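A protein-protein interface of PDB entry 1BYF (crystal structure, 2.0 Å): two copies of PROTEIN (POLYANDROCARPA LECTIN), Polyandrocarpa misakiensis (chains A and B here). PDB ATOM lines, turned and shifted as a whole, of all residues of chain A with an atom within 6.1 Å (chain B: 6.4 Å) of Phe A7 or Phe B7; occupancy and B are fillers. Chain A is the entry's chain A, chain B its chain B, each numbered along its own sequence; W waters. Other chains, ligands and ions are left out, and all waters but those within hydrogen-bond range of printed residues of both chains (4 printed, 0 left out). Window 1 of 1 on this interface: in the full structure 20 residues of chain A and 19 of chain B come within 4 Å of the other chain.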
ATOM      1  N   TYR A   3      -0.745  20.276 -19.450  1.00  0.00           N
ATOM      2  CA  TYR A   3      -0.711  20.194 -18.006  1.00  0.00           C
ATOM      3  C   TYR A   3      -0.001  18.963 -17.458  1.00  0.00           C
ATOM      4  O   TYR A   3       0.387  17.984 -18.076  1.00  0.00           O
ATOM      5  CB  TYR A   3      -2.146  20.043 -17.450  1.00  0.00           C
ATOM      6  CG  TYR A   3      -3.118  21.145 -17.766  1.00  0.00           C
ATOM      7  CD1 TYR A   3      -3.878  21.060 -18.927  1.00  0.00           C
ATOM      8  CD2 TYR A   3      -3.302  22.238 -16.930  1.00  0.00           C
ATOM      9  CE1 TYR A   3      -4.788  22.050 -19.262  1.00  0.00           C
ATOM     10  CE2 TYR A   3      -4.204  23.229 -17.265  1.00  0.00           C
ATOM     11  CZ  TYR A   3      -4.947  23.128 -18.417  1.00  0.00           C
ATOM     12  OH  TYR A   3      -5.836  24.143 -18.695  1.00  0.00           O
ATOM     13  N   GLU A   4       0.074  18.979 -16.139  1.00  0.00           N
ATOM     14  CA  GLU A   4       0.465  17.911 -15.261  1.00  0.00           C
ATOM     15  C   GLU A   4      -0.834  17.601 -14.476  1.00  0.00           C
ATOM     16  O   GLU A   4      -1.403  18.545 -13.931  1.00  0.00           O
ATOM     17  CB  GLU A   4       1.536  18.245 -14.250  1.00  0.00           C
ATOM     18  CG  GLU A   4       2.970  18.100 -14.708  1.00  0.00           C
ATOM     19  CD  GLU A   4       3.945  18.597 -13.664  1.00  0.00           C
ATOM     20  OE1 GLU A   4       3.518  18.876 -12.521  1.00  0.00           O
ATOM     21  OE2 GLU A   4       5.161  18.720 -13.904  1.00  0.00           O
ATOM     22  N   ILE A   5      -1.270  16.361 -14.520  1.00  0.00           N
ATOM     23  CA  ILE A   5      -2.500  15.987 -13.820  1.00  0.00           C
ATOM     24  C   ILE A   5      -2.191  14.857 -12.838  1.00  0.00           C
ATOM     25  O   ILE A   5      -1.620  13.839 -13.215  1.00  0.00           O
ATOM     26  CB  ILE A   5      -3.597  15.538 -14.793  1.00  0.00           C
ATOM     27  CG1 ILE A   5      -3.912  16.641 -15.807  1.00  0.00           C
ATOM     28  CG2 ILE A   5      -4.853  15.107 -14.046  1.00  0.00           C
ATOM     29  CD1 ILE A   5      -4.497  17.913 -15.227  1.00  0.00           C
ATOM     30  N   LEU A   6      -2.552  15.077 -11.584  1.00  0.00           N
ATOM     31  CA  LEU A   6      -2.309  14.082 -10.544  1.00  0.00           C
ATOM     32  C   LEU A   6      -3.649  13.566 -10.019  1.00  0.00           C
ATOM     33  O   LEU A   6      -4.504  14.372  -9.678  1.00  0.00           O
ATOM     34  CB  LEU A   6      -1.491  14.721  -9.422  1.00  0.00           C
ATOM     35  CG  LEU A   6      -1.371  13.948  -8.105  1.00  0.00           C
ATOM     36  CD1 LEU A   6      -0.708  12.596  -8.293  1.00  0.00           C
ATOM     37  CD2 LEU A   6      -0.565  14.752  -7.088  1.00  0.00           C
ATOM     38  N   PHE A   7      -3.846  12.266 -10.002  1.00  0.00           N
ATOM     39  CA  PHE A   7      -5.057  11.648  -9.479  1.00  0.00           C
ATOM     40  C   PHE A   7      -4.657  10.905  -8.200  1.00  0.00           C
ATOM     41  O   PHE A   7      -3.650  10.187  -8.249  1.00  0.00           O
ATOM     42  CB  PHE A   7      -5.664  10.634 -10.436  1.00  0.00           C
ATOM     43  CG  PHE A   7      -6.164  11.149 -11.751  1.00  0.00           C
ATOM     44  CD1 PHE A   7      -5.320  11.239 -12.845  1.00  0.00           C
ATOM     45  CD2 PHE A   7      -7.493  11.515 -11.901  1.00  0.00           C
ATOM     46  CE1 PHE A   7      -5.792  11.702 -14.060  1.00  0.00           C
ATOM     47  CE2 PHE A   7      -7.971  11.975 -13.113  1.00  0.00           C
ATOM     48  CZ  PHE A   7      -7.122  12.072 -14.194  1.00  0.00           C
ATOM     49  N   SER A   8      -5.408  11.044  -7.129  1.00  0.00           N
ATOM     50  CA  SER A   8      -5.063  10.332  -5.901  1.00  0.00           C
ATOM     51  C   SER A   8      -6.253   9.573  -5.325  1.00  0.00           C
ATOM     52  O   SER A   8      -7.362  10.097  -5.232  1.00  0.00           O
ATOM     53  CB  SER A   8      -4.465  11.270  -4.852  1.00  0.00           C
ATOM     54  OG  SER A   8      -4.288  10.549  -3.635  1.00  0.00           O
ATOM     55  N   ASP A   9      -6.004   8.323  -4.954  1.00  0.00           N
ATOM     56  CA  ASP A   9      -7.019   7.470  -4.354  1.00  0.00           C
ATOM     57  C   ASP A   9      -7.274   7.844  -2.895  1.00  0.00           C
ATOM     58  O   ASP A   9      -8.206   7.336  -2.281  1.00  0.00           O
ATOM     59  CB  ASP A   9      -6.617   5.991  -4.425  1.00  0.00           C
ATOM     60  CG  ASP A   9      -6.894   5.446  -5.822  1.00  0.00           C
ATOM     61  OD1 ASP A   9      -7.979   5.769  -6.352  1.00  0.00           O
ATOM     62  OD2 ASP A   9      -6.037   4.714  -6.344  1.00  0.00           O
ATOM     63  N   TYR A  20      -3.718  19.780  -0.142  1.00  0.00           N
ATOM     64  CA  TYR A  20      -3.025  18.603  -0.657  1.00  0.00           C
ATOM     65  C   TYR A  20      -2.339  18.945  -1.976  1.00  0.00           C
ATOM     66  O   TYR A  20      -1.161  18.653  -2.179  1.00  0.00           O
ATOM     67  CB  TYR A  20      -4.039  17.469  -0.844  1.00  0.00           C
ATOM     68  CG  TYR A  20      -3.493  16.205  -1.469  1.00  0.00           C
ATOM     69  CD1 TYR A  20      -3.357  16.101  -2.847  1.00  0.00           C
ATOM     70  CD2 TYR A  20      -3.116  15.119  -0.691  1.00  0.00           C
ATOM     71  CE1 TYR A  20      -2.857  14.957  -3.434  1.00  0.00           C
ATOM     72  CE2 TYR A  20      -2.624  13.961  -1.266  1.00  0.00           C
ATOM     73  CZ  TYR A  20      -2.497  13.892  -2.636  1.00  0.00           C
ATOM     74  OH  TYR A  20      -1.988  12.771  -3.254  1.00  0.00           O
ATOM     75  N   ALA A  41      -9.976  13.465 -21.147  1.00  0.00           N
ATOM     76  CA  ALA A  41      -9.004  12.486 -20.660  1.00  0.00           C
ATOM     77  C   ALA A  41      -9.230  12.254 -19.163  1.00  0.00           C
ATOM     78  O   ALA A  41      -9.227  11.122 -18.670  1.00  0.00           O
ATOM     79  CB  ALA A  41      -7.574  12.954 -20.872  1.00  0.00           C
ATOM     80  N   ILE A  42      -9.411  13.357 -18.448  1.00  0.00           N
ATOM     81  CA  ILE A  42      -9.653  13.322 -17.009  1.00  0.00           C
ATOM     82  C   ILE A  42     -10.908  12.504 -16.726  1.00  0.00           C
ATOM     83  O   ILE A  42     -10.873  11.610 -15.874  1.00  0.00           O
ATOM     84  CB  ILE A  42      -9.752  14.738 -16.406  1.00  0.00           C
ATOM     85  CG1 ILE A  42      -8.365  15.397 -16.317  1.00  0.00           C
ATOM     86  CG2 ILE A  42     -10.391  14.725 -15.022  1.00  0.00           C
ATOM     87  CD1 ILE A  42      -8.397  16.894 -16.071  1.00  0.00           C
ATOM     88  N   LEU A  43     -11.996  12.780 -17.438  1.00  0.00           N
ATOM     89  CA  LEU A  43     -13.242  12.057 -17.223  1.00  0.00           C
ATOM     90  C   LEU A  43     -13.147  10.608 -17.675  1.00  0.00           C
ATOM     91  O   LEU A  43     -13.849   9.768 -17.105  1.00  0.00           O
ATOM     92  CB  LEU A  43     -14.438  12.765 -17.862  1.00  0.00           C
ATOM     93  CG  LEU A  43     -14.909  14.050 -17.168  1.00  0.00           C
ATOM     94  CD1 LEU A  43     -16.055  14.691 -17.943  1.00  0.00           C
ATOM     95  CD2 LEU A  43     -15.337  13.766 -15.731  1.00  0.00           C
ATOM     96  N   PHE A  45     -10.602   8.715 -17.170  1.00  0.00           N
ATOM     97  CA  PHE A  45      -9.950   8.059 -16.041  1.00  0.00           C
ATOM     98  C   PHE A  45     -10.952   7.840 -14.907  1.00  0.00           C
ATOM     99  O   PHE A  45     -11.065   6.748 -14.346  1.00  0.00           O
ATOM    100  CB  PHE A  45      -8.774   8.892 -15.539  1.00  0.00           C
ATOM    101  CG  PHE A  45      -7.913   8.337 -14.445  1.00  0.00           C
ATOM    102  CD1 PHE A  45      -8.319   8.376 -13.117  1.00  0.00           C
ATOM    103  CD2 PHE A  45      -6.679   7.785 -14.727  1.00  0.00           C
ATOM    104  CE1 PHE A  45      -7.512   7.874 -12.108  1.00  0.00           C
ATOM    105  CE2 PHE A  45      -5.861   7.284 -13.728  1.00  0.00           C
ATOM    106  CZ  PHE A  45      -6.279   7.329 -12.412  1.00  0.00           C
ATOM    107  N   THR A  46     -11.659   8.908 -14.528  1.00  0.00           N
ATOM    108  CA  THR A  46     -12.614   8.804 -13.427  1.00  0.00           C
ATOM    109  C   THR A  46     -13.768   7.874 -13.770  1.00  0.00           C
ATOM    110  O   THR A  46     -14.319   7.236 -12.867  1.00  0.00           O
ATOM    111  CB  THR A  46     -13.133  10.174 -12.961  1.00  0.00           C
ATOM    112  OG1 THR A  46     -13.885  10.761 -14.025  1.00  0.00           O
ATOM    113  CG2 THR A  46     -11.958  11.074 -12.594  1.00  0.00           C
ATOM    114  N   TYR A  53     -14.719  12.483  -7.038  1.00  0.00           N
ATOM    115  CA  TYR A  53     -13.495  13.251  -6.971  1.00  0.00           C
ATOM    116  C   TYR A  53     -13.772  14.741  -6.759  1.00  0.00           C
ATOM    117  O   TYR A  53     -14.684  15.267  -7.396  1.00  0.00           O
ATOM    118  CB  TYR A  53     -12.740  13.199  -8.314  1.00  0.00           C
ATOM    119  CG  TYR A  53     -12.072  11.867  -8.554  1.00  0.00           C
ATOM    120  CD1 TYR A  53     -12.796  10.774  -8.997  1.00  0.00           C
ATOM    121  CD2 TYR A  53     -10.712  11.722  -8.326  1.00  0.00           C
ATOM    122  CE1 TYR A  53     -12.178   9.554  -9.213  1.00  0.00           C
ATOM    123  CE2 TYR A  53     -10.081  10.507  -8.542  1.00  0.00           C
ATOM    124  CZ  TYR A  53     -10.825   9.433  -8.979  1.00  0.00           C
ATOM    125  OH  TYR A  53     -10.203   8.222  -9.194  1.00  0.00           O
ATOM    126  N   VAL A 117      -8.979  13.050  -4.971  1.00  0.00           N
ATOM    127  CA  VAL A 117      -8.426  14.331  -5.380  1.00  0.00           C
ATOM    128  C   VAL A 117      -7.760  14.305  -6.749  1.00  0.00           C
ATOM    129  O   VAL A 117      -7.088  13.350  -7.131  1.00  0.00           O
ATOM    130  CB  VAL A 117      -7.384  14.777  -4.327  1.00  0.00           C
ATOM    131  CG1 VAL A 117      -6.840  16.170  -4.645  1.00  0.00           C
ATOM    132  CG2 VAL A 117      -7.997  14.767  -2.924  1.00  0.00           C
ATOM    133  N   ILE A 118      -7.941  15.403  -7.467  1.00  0.00           N
ATOM    134  CA  ILE A 118      -7.356  15.631  -8.771  1.00  0.00           C
ATOM    135  C   ILE A 118      -6.667  16.998  -8.750  1.00  0.00           C
ATOM    136  O   ILE A 118      -7.326  18.004  -8.481  1.00  0.00           O
ATOM    137  CB  ILE A 118      -8.378  15.640  -9.920  1.00  0.00           C
ATOM    138  CG1 ILE A 118      -9.213  14.359  -9.871  1.00  0.00           C
ATOM    139  CG2 ILE A 118      -7.671  15.776 -11.265  1.00  0.00           C
ATOM    140  CD1 ILE A 118     -10.356  14.347 -10.868  1.00  0.00           C
ATOM    141  N   CYS A 119      -5.366  16.995  -9.010  1.00  0.00           N
ATOM    142  CA  CYS A 119      -4.608  18.232  -9.047  1.00  0.00           C
ATOM    143  C   CYS A 119      -4.090  18.488 -10.466  1.00  0.00           C
ATOM    144  O   CYS A 119      -3.922  17.552 -11.251  1.00  0.00           O
ATOM    145  CB  CYS A 119      -3.397  18.203  -8.121  1.00  0.00           C
ATOM    146  SG  CYS A 119      -3.723  17.609  -6.456  1.00  0.00           S
ATOM    147  N   TYR B   3      -3.225   4.045  -5.599  1.00  0.00           N
ATOM    148  CA  TYR B   3      -2.146   4.902  -6.026  1.00  0.00           C
ATOM    149  C   TYR B   3      -2.415   6.393  -6.149  1.00  0.00           C
ATOM    150  O   TYR B   3      -3.492   6.966  -6.147  1.00  0.00           O
ATOM    151  CB  TYR B   3      -1.759   4.491  -7.478  1.00  0.00           C
ATOM    152  CG  TYR B   3      -1.241   3.080  -7.590  1.00  0.00           C
ATOM    153  CD1 TYR B   3      -2.142   2.031  -7.739  1.00  0.00           C
ATOM    154  CD2 TYR B   3       0.114   2.785  -7.551  1.00  0.00           C
ATOM    155  CE1 TYR B   3      -1.708   0.725  -7.844  1.00  0.00           C
ATOM    156  CE2 TYR B   3       0.555   1.476  -7.656  1.00  0.00           C
ATOM    157  CZ  TYR B   3      -0.359   0.455  -7.803  1.00  0.00           C
ATOM    158  OH  TYR B   3       0.097  -0.839  -7.899  1.00  0.00           O
ATOM    159  N   GLU B   4      -1.289   7.059  -6.370  1.00  0.00           N
ATOM    160  CA  GLU B   4      -1.133   8.426  -6.784  1.00  0.00           C
ATOM    161  C   GLU B   4      -0.558   8.281  -8.215  1.00  0.00           C
ATOM    162  O   GLU B   4       0.500   7.678  -8.355  1.00  0.00           O
ATOM    163  CB  GLU B   4      -0.145   9.254  -5.994  1.00  0.00           C
ATOM    164  CG  GLU B   4      -0.745  10.153  -4.927  1.00  0.00           C
ATOM    165  CD  GLU B   4       0.356  10.835  -4.135  1.00  0.00           C
ATOM    166  OE1 GLU B   4       1.480  10.964  -4.669  1.00  0.00           O
ATOM    167  OE2 GLU B   4       0.132  11.249  -2.983  1.00  0.00           O
ATOM    168  N   ILE B   5      -1.300   8.753  -9.190  1.00  0.00           N
ATOM    169  CA  ILE B   5      -0.837   8.661 -10.570  1.00  0.00           C
ATOM    170  C   ILE B   5      -0.686  10.079 -11.125  1.00  0.00           C
ATOM    171  O   ILE B   5      -1.621  10.875 -11.068  1.00  0.00           O
ATOM    172  CB  ILE B   5      -1.780   7.862 -11.477  1.00  0.00           C
ATOM    173  CG1 ILE B   5      -1.991   6.444 -10.950  1.00  0.00           C
ATOM    174  CG2 ILE B   5      -1.251   7.829 -12.906  1.00  0.00           C
ATOM    175  CD1 ILE B   5      -0.753   5.572 -10.870  1.00  0.00           C
ATOM    176  N   LEU B   6       0.504  10.354 -11.642  1.00  0.00           N
ATOM    177  CA  LEU B   6       0.805  11.652 -12.218  1.00  0.00           C
ATOM    178  C   LEU B   6       1.041  11.531 -13.724  1.00  0.00           C
ATOM    179  O   LEU B   6       1.872  10.720 -14.130  1.00  0.00           O
ATOM    180  CB  LEU B   6       2.068  12.196 -11.541  1.00  0.00           C
ATOM    181  CG  LEU B   6       2.701  13.445 -12.147  1.00  0.00           C
ATOM    182  CD1 LEU B   6       1.797  14.655 -11.974  1.00  0.00           C
ATOM    183  CD2 LEU B   6       4.059  13.743 -11.514  1.00  0.00           C
ATOM    184  N   PHE B   7       0.318  12.289 -14.532  1.00  0.00           N
ATOM    185  CA  PHE B   7       0.507  12.298 -15.976  1.00  0.00           C
ATOM    186  C   PHE B   7       1.129  13.654 -16.348  1.00  0.00           C
ATOM    187  O   PHE B   7       0.630  14.677 -15.864  1.00  0.00           O
ATOM    188  CB  PHE B   7      -0.784  12.173 -16.785  1.00  0.00           C
ATOM    189  CG  PHE B   7      -1.521  10.870 -16.664  1.00  0.00           C
ATOM    190  CD1 PHE B   7      -2.474  10.696 -15.678  1.00  0.00           C
ATOM    191  CD2 PHE B   7      -1.271   9.830 -17.545  1.00  0.00           C
ATOM    192  CE1 PHE B   7      -3.163   9.502 -15.561  1.00  0.00           C
ATOM    193  CE2 PHE B   7      -1.964   8.634 -17.447  1.00  0.00           C
ATOM    194  CZ  PHE B   7      -2.908   8.469 -16.448  1.00  0.00           C
ATOM    195  N   SER B   8       2.168  13.661 -17.174  1.00  0.00           N
ATOM    196  CA  SER B   8       2.763  14.935 -17.563  1.00  0.00           C
ATOM    197  C   SER B   8       2.847  15.082 -19.076  1.00  0.00           C
ATOM    198  O   SER B   8       3.305  14.180 -19.778  1.00  0.00           O
ATOM    199  CB  SER B   8       4.162  15.132 -16.975  1.00  0.00           C
ATOM    200  OG  SER B   8       4.742  16.309 -17.527  1.00  0.00           O
ATOM    201  N   ASP B   9       2.431  16.248 -19.563  1.00  0.00           N
ATOM    202  CA  ASP B   9       2.514  16.534 -20.988  1.00  0.00           C
ATOM    203  C   ASP B   9       3.950  16.872 -21.392  1.00  0.00           C
ATOM    204  O   ASP B   9       4.241  16.913 -22.591  1.00  0.00           O
ATOM    205  CB  ASP B   9       1.574  17.676 -21.360  1.00  0.00           C
ATOM    206  CG  ASP B   9       0.150  17.209 -21.606  1.00  0.00           C
ATOM    207  OD1 ASP B   9      -0.053  16.132 -22.206  1.00  0.00           O
ATOM    208  OD2 ASP B   9      -0.764  17.957 -21.203  1.00  0.00           O
ATOM    209  N   TYR B  20      12.674  12.327 -13.280  1.00  0.00           N
ATOM    210  CA  TYR B  20      11.560  13.260 -13.126  1.00  0.00           C
ATOM    211  C   TYR B  20      10.605  12.725 -12.060  1.00  0.00           C
ATOM    212  O   TYR B  20      10.213  13.464 -11.162  1.00  0.00           O
ATOM    213  CB  TYR B  20      10.872  13.515 -14.460  1.00  0.00           C
ATOM    214  CG  TYR B  20       9.533  14.211 -14.400  1.00  0.00           C
ATOM    215  CD1 TYR B  20       8.381  13.487 -14.111  1.00  0.00           C
ATOM    216  CD2 TYR B  20       9.399  15.569 -14.638  1.00  0.00           C
ATOM    217  CE1 TYR B  20       7.145  14.092 -14.048  1.00  0.00           C
ATOM    218  CE2 TYR B  20       8.160  16.185 -14.581  1.00  0.00           C
ATOM    219  CZ  TYR B  20       7.037  15.444 -14.283  1.00  0.00           C
ATOM    220  OH  TYR B  20       5.802  16.051 -14.215  1.00  0.00           O
ATOM    221  N   ALA B  41      -7.794   2.474 -15.971  1.00  0.00           N
ATOM    222  CA  ALA B  41      -7.978   3.916 -15.852  1.00  0.00           C
ATOM    223  C   ALA B  41      -6.841   4.684 -16.526  1.00  0.00           C
ATOM    224  O   ALA B  41      -7.076   5.677 -17.217  1.00  0.00           O
ATOM    225  CB  ALA B  41      -8.092   4.325 -14.387  1.00  0.00           C
ATOM    226  N   ILE B  42      -5.614   4.216 -16.326  1.00  0.00           N
ATOM    227  CA  ILE B  42      -4.449   4.834 -16.949  1.00  0.00           C
ATOM    228  C   ILE B  42      -4.598   4.818 -18.468  1.00  0.00           C
ATOM    229  O   ILE B  42      -4.448   5.860 -19.094  1.00  0.00           O
ATOM    230  CB  ILE B  42      -3.136   4.130 -16.543  1.00  0.00           C
ATOM    231  CG1 ILE B  42      -2.913   4.319 -15.042  1.00  0.00           C
ATOM    232  CG2 ILE B  42      -1.951   4.656 -17.352  1.00  0.00           C
ATOM    233  CD1 ILE B  42      -1.793   3.482 -14.459  1.00  0.00           C
ATOM    234  N   LEU B  43      -4.904   3.658 -19.041  1.00  0.00           N
ATOM    235  CA  LEU B  43      -5.043   3.553 -20.489  1.00  0.00           C
ATOM    236  C   LEU B  43      -6.233   4.351 -21.000  1.00  0.00           C
ATOM    237  O   LEU B  43      -6.194   4.822 -22.137  1.00  0.00           O
ATOM    238  CB  LEU B  43      -5.095   2.081 -20.924  1.00  0.00           C
ATOM    239  CG  LEU B  43      -3.805   1.276 -20.700  1.00  0.00           C
ATOM    240  CD1 LEU B  43      -4.023  -0.199 -21.018  1.00  0.00           C
ATOM    241  CD2 LEU B  43      -2.656   1.846 -21.527  1.00  0.00           C
ATOM    242  N   PHE B  45      -7.138   7.268 -19.931  1.00  0.00           N
ATOM    243  CA  PHE B  45      -6.621   8.631 -20.036  1.00  0.00           C
ATOM    244  C   PHE B  45      -5.734   8.790 -21.276  1.00  0.00           C
ATOM    245  O   PHE B  45      -5.923   9.717 -22.067  1.00  0.00           O
ATOM    246  CB  PHE B  45      -5.830   8.940 -18.767  1.00  0.00           C
ATOM    247  CG  PHE B  45      -5.293  10.336 -18.672  1.00  0.00           C
ATOM    248  CD1 PHE B  45      -4.098  10.682 -19.276  1.00  0.00           C
ATOM    249  CD2 PHE B  45      -5.980  11.300 -17.948  1.00  0.00           C
ATOM    250  CE1 PHE B  45      -3.588  11.963 -19.169  1.00  0.00           C
ATOM    251  CE2 PHE B  45      -5.475  12.584 -17.844  1.00  0.00           C
ATOM    252  CZ  PHE B  45      -4.285  12.913 -18.449  1.00  0.00           C
ATOM    253  N   THR B  46      -4.743   7.907 -21.419  1.00  0.00           N
ATOM    254  CA  THR B  46      -3.826   7.990 -22.555  1.00  0.00           C
ATOM    255  C   THR B  46      -4.536   7.774 -23.880  1.00  0.00           C
ATOM    256  O   THR B  46      -4.097   8.294 -24.914  1.00  0.00           O
ATOM    257  CB  THR B  46      -2.633   7.029 -22.402  1.00  0.00           C
ATOM    258  OG1 THR B  46      -3.094   5.673 -22.360  1.00  0.00           O
ATOM    259  CG2 THR B  46      -1.875   7.322 -21.108  1.00  0.00           C
ATOM    260  N   TYR B  53       3.698   7.563 -24.214  1.00  0.00           N
ATOM    261  CA  TYR B  53       4.100   7.792 -22.832  1.00  0.00           C
ATOM    262  C   TYR B  53       5.139   6.772 -22.373  1.00  0.00           C
ATOM    263  O   TYR B  53       4.981   5.594 -22.691  1.00  0.00           O
ATOM    264  CB  TYR B  53       2.903   7.635 -21.881  1.00  0.00           C
ATOM    265  CG  TYR B  53       1.880   8.741 -21.940  1.00  0.00           C
ATOM    266  CD1 TYR B  53       0.921   8.772 -22.938  1.00  0.00           C
ATOM    267  CD2 TYR B  53       1.868   9.751 -20.986  1.00  0.00           C
ATOM    268  CE1 TYR B  53      -0.022   9.786 -22.998  1.00  0.00           C
ATOM    269  CE2 TYR B  53       0.926  10.767 -21.033  1.00  0.00           C
ATOM    270  CZ  TYR B  53      -0.006  10.779 -22.044  1.00  0.00           C
ATOM    271  OH  TYR B  53      -0.955  11.779 -22.089  1.00  0.00           O
ATOM    272  N   VAL B 117       5.309  11.426 -19.700  1.00  0.00           N
ATOM    273  CA  VAL B 117       5.645  10.692 -18.501  1.00  0.00           C
ATOM    274  C   VAL B 117       4.443  10.379 -17.616  1.00  0.00           C
ATOM    275  O   VAL B 117       3.567  11.212 -17.433  1.00  0.00           O
ATOM    276  CB  VAL B 117       6.655  11.505 -17.653  1.00  0.00           C
ATOM    277  CG1 VAL B 117       7.061  10.759 -16.391  1.00  0.00           C
ATOM    278  CG2 VAL B 117       7.887  11.847 -18.478  1.00  0.00           C
ATOM    279  N   ILE B 118       4.468   9.176 -17.063  1.00  0.00           N
ATOM    280  CA  ILE B 118       3.479   8.729 -16.102  1.00  0.00           C
ATOM    281  C   ILE B 118       4.233   8.228 -14.862  1.00  0.00           C
ATOM    282  O   ILE B 118       5.089   7.348 -14.981  1.00  0.00           O
ATOM    283  CB  ILE B 118       2.570   7.594 -16.607  1.00  0.00           C
ATOM    284  CG1 ILE B 118       1.927   7.946 -17.952  1.00  0.00           C
ATOM    285  CG2 ILE B 118       1.489   7.300 -15.564  1.00  0.00           C
ATOM    286  CD1 ILE B 118       1.213   6.782 -18.615  1.00  0.00           C
ATOM    287  N   CYS B 119       3.911   8.805 -13.708  1.00  0.00           N
ATOM    288  CA  CYS B 119       4.528   8.399 -12.460  1.00  0.00           C
ATOM    289  C   CYS B 119       3.469   7.800 -11.528  1.00  0.00           C
ATOM    290  O   CYS B 119       2.283   8.112 -11.651  1.00  0.00           O
ATOM    291  CB  CYS B 119       5.189   9.564 -11.716  1.00  0.00           C
ATOM    292  SG  CYS B 119       6.302  10.588 -12.687  1.00  0.00           S
HETATM  293  O   HOH W   1      -2.176  10.668  -1.799  1.00  0.00           O
HETATM  294  O   HOH W   2      -4.966   7.333  -8.714  1.00  0.00           O
HETATM  295  O   HOH W   3      -1.196  15.447 -18.263  1.00  0.00           O
HETATM  296  O   HOH W   4       6.148  18.119 -16.161  1.00  0.00           O
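Among the printed residues, merely in contact across the chains: Tyr A3 with Phe B7, Tyr A3 with Ser B8, Glu A4 with Phe B7, Glu A4 with Ser B8, Ile A5 with Ile B5, Ile A5 with Leu B6, Leu A6 with Ile B5, Phe A7 with Tyr B3, Phe A7 with Glu B4, Phe A7 with Phe B7, Phe A7 with Phe B45, Ser A8 with Tyr B3, Ser A8 with Glu B4, Ala A41 with Phe B45, Phe A45 with Phe B7 and Phe A45 with Ala B41.
O of Leu A6 lies within hydrogen-bond range of N of Cys A119 (2.8 Å). OG of Ser A8 sits at hydrogen-bond distance from OH of Tyr A20 (3.2 Å). O of Val A117 lies within hydrogen-bond range of N of Ser A8. The backbone NH of Cys B119 sits at hydrogen-bond distance from the backbone carbonyl oxygen of Leu B6, 2.8 Å away. The side-chain hydroxyl of Tyr B20 lies close to the side-chain hydroxyl of Ser B8 (3.5 Å). The backbone carbonyl oxygen of Val B117 sits at hydrogen-bond distance from the backbone NH of Ser B8 (2.8 Å).
Hydrophobic or aromatic side chains of chain B that line the printed part of chain A: Leu B6, Phe B7, Tyr B20, Ala B41 and Phe B45. Hydrophobic or aromatic side chains of chain A within 4 Å of the printed part of chain B: Leu A6, Phe A7, Tyr A20, Ala A41 and Phe A45. Along chain A the printed residues that touch a printed residue of chain B span positions 3 to 45. Among the printed residues, 22 pairs touch across the chains. Among the printed residues, no Asp or Glu carboxylate lies within 4 Å of a Lys or Arg side-chain nitrogen of the other chain.
The backbone NH of Tyr A3 is in hydrogen-bond range of the side-chain carboxylate of Asp B9 (2.9 Å). The side-chain carboxylate (OE2) of Glu A4 is in hydrogen-bond range of the side-chain hydroxyl (OH) of Tyr B20 (2.8 Å). The backbone carbonyl oxygen (O) of Ile A5 sits at hydrogen-bond distance from the backbone NH (N) of Phe B7 (2.8 Å). The backbone NH (N) of Phe A7 sits at hydrogen-bond distance from the backbone carbonyl oxygen (O) of Ile B5, at 2.8 Å. The side-chain carboxylate of Asp A9 sits at hydrogen-bond distance from the backbone NH of Tyr B3 (3.0 Å). OE2 of Glu B4 lies within hydrogen-bond range of OH of Tyr A20 (2.6 Å).
Tyr A3 touches Asp B9, and with the chains exchanged Asp A9 touches Tyr B3. Ile B5 touches its own counterpart, Ile A5. Ile A5 touches Phe B7, and with the chains exchanged Phe A7 touches Ile B5. Ala A41 touches Phe B45, and with the chains exchanged Phe A45 touches Ala B41.
Water W4 lies within hydrogen-bond range of OE2 of Glu A4, OG of Ser B8 and OH of Tyr B20. Water W1 lies within hydrogen-bond range of the side-chain hydroxyl (OH) of Tyr A20, the side-chain carboxylate (OE2) of Glu B4 and the side-chain hydroxyl (OG) of Ser A8. Water W2 lies within hydrogen-bond range of the backbone carbonyl oxygen of Tyr B3 and the backbone carbonyl oxygen of Phe A7. Water W3 lies within hydrogen-bond range of the backbone carbonyl oxygen of Tyr A3 and the backbone carbonyl oxygen of Phe B7.
Of chain B, only Tyr B3, Glu B4, Ile B5, Phe B7 and Phe B45 come within 4 Å of Phe A7. Of the printed residues of chain B, Phe A45 touches Phe B7 and Ala B41. Thr A46 touches none of the printed residues of chain B. Val A117 touches none of the printed residues of chain B. Of the printed residues of chain A, Tyr B3 touches Phe A7, Ser A8 and Asp A9. Of the printed residues of chain A, Asp B9 touches Tyr A3 (2.9 Å). Of the printed residues of chain A, Tyr B20 touches Glu A4. The nearest residue of chain B that does not touch Phe A7 is Leu B6 (5.0 Å). The nearest printed residue of chain A that does not touch Phe B7 is Leu A6 (5.0 Å). The nearest printed residue of chain A that does not touch Ser B8 is Ile A5 (5.1 Å).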
